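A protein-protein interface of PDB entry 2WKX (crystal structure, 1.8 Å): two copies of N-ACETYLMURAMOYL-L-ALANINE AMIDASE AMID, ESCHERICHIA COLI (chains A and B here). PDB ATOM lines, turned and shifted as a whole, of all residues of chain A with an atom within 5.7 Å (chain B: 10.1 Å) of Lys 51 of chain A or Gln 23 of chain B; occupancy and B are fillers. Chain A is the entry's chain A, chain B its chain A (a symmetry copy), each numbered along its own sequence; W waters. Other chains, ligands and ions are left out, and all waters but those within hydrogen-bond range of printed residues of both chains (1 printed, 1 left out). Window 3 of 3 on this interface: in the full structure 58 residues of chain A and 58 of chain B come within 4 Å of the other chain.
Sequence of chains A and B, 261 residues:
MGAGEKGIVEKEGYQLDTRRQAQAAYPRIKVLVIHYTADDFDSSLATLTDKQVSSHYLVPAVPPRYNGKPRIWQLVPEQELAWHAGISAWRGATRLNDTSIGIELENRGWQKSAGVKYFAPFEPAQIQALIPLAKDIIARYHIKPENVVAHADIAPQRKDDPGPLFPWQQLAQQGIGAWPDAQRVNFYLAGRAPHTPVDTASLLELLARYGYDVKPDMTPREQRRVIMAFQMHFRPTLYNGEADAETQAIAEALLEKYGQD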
ATOM      1  N   THR A  47     -10.932  -5.624  11.454  1.00  0.00           N
ATOM      2  CA  THR A  47     -10.174  -6.316  12.499  1.00  0.00           C
ATOM      3  C   THR A  47     -11.097  -6.961  13.533  1.00  0.00           C
ATOM      4  O   THR A  47     -10.919  -8.142  13.903  1.00  0.00           O
ATOM      5  CB  THR A  47      -9.170  -5.351  13.175  1.00  0.00           C
ATOM      6  OG1 THR A  47      -8.190  -4.960  12.208  1.00  0.00           O
ATOM      7  CG2 THR A  47      -8.464  -6.003  14.338  1.00  0.00           C
ATOM      8  N   LEU A  48     -12.083  -6.192  13.998  1.00  0.00           N
ATOM      9  CA  LEU A  48     -12.911  -6.607  15.136  1.00  0.00           C
ATOM     10  C   LEU A  48     -13.972  -7.644  14.758  1.00  0.00           C
ATOM     11  O   LEU A  48     -14.675  -8.172  15.621  1.00  0.00           O
ATOM     12  CB  LEU A  48     -13.554  -5.392  15.801  1.00  0.00           C
ATOM     13  CG  LEU A  48     -12.552  -4.538  16.601  1.00  0.00           C
ATOM     14  CD1 LEU A  48     -13.176  -3.162  16.879  1.00  0.00           C
ATOM     15  CD2 LEU A  48     -12.111  -5.223  17.918  1.00  0.00           C
ATOM     16  N   THR A  49     -14.067  -7.927  13.461  1.00  0.00           N
ATOM     17  CA  THR A  49     -14.936  -8.996  12.970  1.00  0.00           C
ATOM     18  C   THR A  49     -14.116 -10.184  12.407  1.00  0.00           C
ATOM     19  O   THR A  49     -14.711 -11.101  11.835  1.00  0.00           O
ATOM     20  CB  THR A  49     -16.010  -8.469  11.950  1.00  0.00           C
ATOM     21  OG1 THR A  49     -15.368  -7.801  10.856  1.00  0.00           O
ATOM     22  CG2 THR A  49     -16.984  -7.505  12.627  1.00  0.00           C
ATOM     23  N   ASP A  50     -12.785 -10.172  12.581  1.00  0.00           N
ATOM     24  CA  ASP A  50     -11.878 -11.244  12.097  1.00  0.00           C
ATOM     25  C   ASP A  50     -11.821 -12.450  13.052  1.00  0.00           C
ATOM     26  O   ASP A  50     -12.626 -12.549  13.983  1.00  0.00           O
ATOM     27  CB  ASP A  50     -10.472 -10.739  11.674  1.00  0.00           C
ATOM     28  CG  ASP A  50      -9.488 -10.434  12.850  1.00  0.00           C
ATOM     29  OD1 ASP A  50      -9.689 -10.773  14.040  1.00  0.00           O
ATOM     30  OD2 ASP A  50      -8.440  -9.809  12.558  1.00  0.00           O
ATOM     31  N   LYS A  51     -10.885 -13.363  12.811  1.00  0.00           N
ATOM     32  CA  LYS A  51     -10.830 -14.606  13.591  1.00  0.00           C
ATOM     33  C   LYS A  51     -10.118 -14.472  14.941  1.00  0.00           C
ATOM     34  O   LYS A  51     -10.235 -15.363  15.781  1.00  0.00           O
ATOM     35  CB  LYS A  51     -10.201 -15.735  12.763  1.00  0.00           C
ATOM     36  CG  LYS A  51     -11.097 -16.249  11.632  1.00  0.00           C
ATOM     37  CD  LYS A  51     -10.478 -17.438  10.883  1.00  0.00           C
ATOM     38  CE  LYS A  51      -9.329 -17.003   9.973  1.00  0.00           C
ATOM     39  NZ  LYS A  51      -8.992 -18.052   8.959  1.00  0.00           N
ATOM     40  N   GLN A  52      -9.416 -13.361  15.156  1.00  0.00           N
ATOM     41  CA  GLN A  52      -8.511 -13.259  16.306  1.00  0.00           C
ATOM     42  C   GLN A  52      -8.930 -12.339  17.449  1.00  0.00           C
ATOM     43  O   GLN A  52      -8.475 -12.535  18.588  1.00  0.00           O
ATOM     44  CB  GLN A  52      -7.122 -12.853  15.818  1.00  0.00           C
ATOM     45  CG  GLN A  52      -6.473 -13.922  14.937  1.00  0.00           C
ATOM     46  CD  GLN A  52      -5.256 -13.423  14.192  1.00  0.00           C
ATOM     47  OE1 GLN A  52      -4.520 -12.556  14.674  1.00  0.00           O
ATOM     48  NE2 GLN A  52      -5.032 -13.976  13.004  1.00  0.00           N
ATOM     49  N   VAL A  53      -9.774 -11.351  17.144  1.00  0.00           N
ATOM     50  CA  VAL A  53     -10.163 -10.311  18.104  1.00  0.00           C
ATOM     51  C   VAL A  53     -11.586  -9.814  17.793  1.00  0.00           C
ATOM     52  O   VAL A  53     -12.043  -9.904  16.649  1.00  0.00           O
ATOM     53  CB  VAL A  53      -9.092  -9.161  18.098  1.00  0.00           C
ATOM     54  CG1 VAL A  53      -9.022  -8.461  16.747  1.00  0.00           C
ATOM     55  CG2 VAL A  53      -9.306  -8.131  19.202  1.00  0.00           C
ATOM     56  N   TRP A  83     -13.570 -11.263  22.115  1.00  0.00           N
ATOM     57  CA  TRP A  83     -12.142 -11.453  22.395  1.00  0.00           C
ATOM     58  C   TRP A  83     -11.455 -10.088  22.405  1.00  0.00           C
ATOM     59  O   TRP A  83     -10.810  -9.720  21.425  1.00  0.00           O
ATOM     60  CB  TRP A  83     -11.520 -12.383  21.343  1.00  0.00           C
ATOM     61  CG  TRP A  83     -11.703 -13.864  21.643  1.00  0.00           C
ATOM     62  CD1 TRP A  83     -12.263 -14.432  22.767  1.00  0.00           C
ATOM     63  CD2 TRP A  83     -11.256 -14.953  20.827  1.00  0.00           C
ATOM     64  NE1 TRP A  83     -12.202 -15.814  22.681  1.00  0.00           N
ATOM     65  CE2 TRP A  83     -11.592 -16.154  21.500  1.00  0.00           C
ATOM     66  CE3 TRP A  83     -10.600 -15.030  19.587  1.00  0.00           C
ATOM     67  CZ2 TRP A  83     -11.297 -17.420  20.970  1.00  0.00           C
ATOM     68  CZ3 TRP A  83     -10.315 -16.287  19.059  1.00  0.00           C
ATOM     69  CH2 TRP A  83     -10.667 -17.464  19.749  1.00  0.00           C
ATOM     70  N   ARG B  20     -23.210  -6.049  11.071  1.00  0.00           N
ATOM     71  CA  ARG B  20     -21.923  -6.717  10.982  1.00  0.00           C
ATOM     72  C   ARG B  20     -21.671  -7.525  12.251  1.00  0.00           C
ATOM     73  O   ARG B  20     -21.524  -6.949  13.334  1.00  0.00           O
ATOM     74  CB  ARG B  20     -20.811  -5.687  10.755  1.00  0.00           C
ATOM     75  CG  ARG B  20     -20.914  -4.913   9.422  1.00  0.00           C
ATOM     76  CD  ARG B  20     -20.667  -5.821   8.203  1.00  0.00           C
ATOM     77  NE  ARG B  20     -19.534  -6.720   8.454  1.00  0.00           N
ATOM     78  CZ  ARG B  20     -18.250  -6.399   8.285  1.00  0.00           C
ATOM     79  NH1 ARG B  20     -17.903  -5.196   7.835  1.00  0.00           N
ATOM     80  NH2 ARG B  20     -17.301  -7.289   8.561  1.00  0.00           N
ATOM     81  N   GLN B  21     -21.609  -8.846  12.115  1.00  0.00           N
ATOM     82  CA  GLN B  21     -21.372  -9.741  13.262  1.00  0.00           C
ATOM     83  C   GLN B  21     -19.925 -10.230  13.300  1.00  0.00           C
ATOM     84  O   GLN B  21     -19.416 -10.698  12.282  1.00  0.00           O
ATOM     85  CB  GLN B  21     -22.288 -10.971  13.201  1.00  0.00           C
ATOM     86  CG  GLN B  21     -23.776 -10.697  13.081  1.00  0.00           C
ATOM     87  CD  GLN B  21     -24.565 -11.956  12.730  1.00  0.00           C
ATOM     88  OE1 GLN B  21     -24.761 -12.838  13.574  1.00  0.00           O
ATOM     89  NE2 GLN B  21     -25.026 -12.041  11.480  1.00  0.00           N
ATOM     90  N   ALA B  22     -19.274 -10.147  14.466  1.00  0.00           N
ATOM     91  CA  ALA B  22     -17.918 -10.663  14.639  1.00  0.00           C
ATOM     92  C   ALA B  22     -17.904 -12.189  14.595  1.00  0.00           C
ATOM     93  O   ALA B  22     -18.837 -12.847  15.087  1.00  0.00           O
ATOM     94  CB  ALA B  22     -17.336 -10.199  15.983  1.00  0.00           C
ATOM     95  N   GLN B  23     -16.835 -12.753  14.037  1.00  0.00           N
ATOM     96  CA  GLN B  23     -16.638 -14.213  14.099  1.00  0.00           C
ATOM     97  C   GLN B  23     -16.241 -14.690  15.495  1.00  0.00           C
ATOM     98  O   GLN B  23     -16.636 -15.792  15.908  1.00  0.00           O
ATOM     99  CB  GLN B  23     -15.547 -14.662  13.134  1.00  0.00           C
ATOM    100  CG  GLN B  23     -15.827 -14.403  11.681  1.00  0.00           C
ATOM    101  CD  GLN B  23     -14.622 -14.764  10.840  1.00  0.00           C
ATOM    102  OE1 GLN B  23     -14.308 -15.943  10.667  1.00  0.00           O
ATOM    103  NE2 GLN B  23     -13.929 -13.754  10.328  1.00  0.00           N
ATOM    104  N   ALA B  24     -15.459 -13.875  16.207  1.00  0.00           N
ATOM    105  CA  ALA B  24     -14.992 -14.258  17.552  1.00  0.00           C
ATOM    106  C   ALA B  24     -16.073 -13.904  18.576  1.00  0.00           C
ATOM    107  O   ALA B  24     -16.068 -12.832  19.188  1.00  0.00           O
ATOM    108  CB  ALA B  24     -13.658 -13.593  17.874  1.00  0.00           C
ATOM    109  N   ALA B  25     -17.039 -14.814  18.712  1.00  0.00           N
ATOM    110  CA  ALA B  25     -18.144 -14.668  19.646  1.00  0.00           C
ATOM    111  C   ALA B  25     -18.411 -16.071  20.166  1.00  0.00           C
ATOM    112  O   ALA B  25     -18.708 -16.990  19.372  1.00  0.00           O
ATOM    113  CB  ALA B  25     -19.368 -14.121  18.953  1.00  0.00           C
ATOM    114  N   TYR B  26     -18.332 -16.225  21.487  1.00  0.00           N
ATOM    115  CA  TYR B  26     -18.416 -17.544  22.123  1.00  0.00           C
ATOM    116  C   TYR B  26     -19.247 -17.501  23.402  1.00  0.00           C
ATOM    117  O   TYR B  26     -19.365 -16.423  24.014  1.00  0.00           O
ATOM    118  CB  TYR B  26     -17.006 -18.065  22.443  1.00  0.00           C
ATOM    119  CG  TYR B  26     -16.141 -18.169  21.204  1.00  0.00           C
ATOM    120  CD1 TYR B  26     -15.242 -17.150  20.872  1.00  0.00           C
ATOM    121  CD2 TYR B  26     -16.246 -19.273  20.344  1.00  0.00           C
ATOM    122  CE1 TYR B  26     -14.455 -17.232  19.698  1.00  0.00           C
ATOM    123  CE2 TYR B  26     -15.467 -19.364  19.179  1.00  0.00           C
ATOM    124  CZ  TYR B  26     -14.578 -18.335  18.874  1.00  0.00           C
ATOM    125  OH  TYR B  26     -13.804 -18.418  17.744  1.00  0.00           O
ATOM    126  N   PRO B  27     -19.801 -18.663  23.827  1.00  0.00           N
ATOM    127  CA  PRO B  27     -20.541 -18.700  25.092  1.00  0.00           C
ATOM    128  C   PRO B  27     -19.664 -18.279  26.268  1.00  0.00           C
ATOM    129  O   PRO B  27     -18.455 -18.558  26.278  1.00  0.00           O
ATOM    130  CB  PRO B  27     -20.963 -20.176  25.230  1.00  0.00           C
ATOM    131  CG  PRO B  27     -20.948 -20.719  23.808  1.00  0.00           C
ATOM    132  CD  PRO B  27     -19.797 -19.976  23.148  1.00  0.00           C
HETATM  133  O   HOH W   1     -12.823 -16.751  15.918  1.00  0.00           O
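OD1 of Asp 50 of chain A sits at hydrogen-bond distance from N of Gln 52 of chain A.
The side-chain carboxylate of Asp 50 of chain A sits at hydrogen-bond distance from the backbone NH of Val 53 of chain A.
Hydrophobic or aromatic side chains of chain B that line the printed part of chain A: Ala 22, Ala 24 and Tyr 26.
Of the 8 printed residues of chain A, 5 touch a printed residue of chain B.
Along chain A the printed residues that touch a printed residue of chain B span positions 48 to 83.
Among the printed residues, 9 pairs touch across the chains.
Among the printed residues, no Asp or Glu carboxylate lies within 4 Å of a Lys or Arg side-chain nitrogen of the other chain.
OG1 of Thr 49 of chain A sits at hydrogen-bond distance from NH2 of Arg 20 of chain B.
The side-chain amide nitrogen (NE2) of Gln 23 of chain B sits at hydrogen-bond distance from the backbone carbonyl oxygen (O) of Thr 49 of chain A (3.1 Å).
Among the printed residues, pairs that only touch across the chains: Leu 48 of chain A with Ala 22 of chain B, Lys 51 of chain A with Gln 23 of chain B, Trp 83 of chain A with Tyr 26 of chain B, Asp 50 of chain A with Gln 23 of chain B, Trp 83 of chain A with Ala 24 of chain B, Thr 49 of chain A with Ala 22 of chain B and Asp 50 of chain A with Ala 24 of chain B.
No position is printed for both chains.
Of the printed residues of chain B, Leu 48 of chain A touches Ala 22.
Of the printed residues of chain B, Thr 49 of chain A touches Arg 20 (3.0 Å), Ala 22 (3.8 Å) and Gln 23 (3.1 Å).
Of chain B, only Gln 23 and Ala 24 come within 4 Å of Asp 50 of chain A.
Of chain B, only Gln 23 comes within 4 Å of Lys 51 of chain A.
Gln 52 of chain A touches none of the printed residues of chain B.
Printed residues of chain B within 4 Å of Trp 83 of chain A: Ala 24 (3.8 Å) and Tyr 26 (3.4 Å).
Of chain A, only Thr 49, Asp 50 and Lys 51 come within 4 Å of Gln 23 of chain B.
Water W1 bridges OH of Tyr 26 of chain B and O of Lys 51 of chain A.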
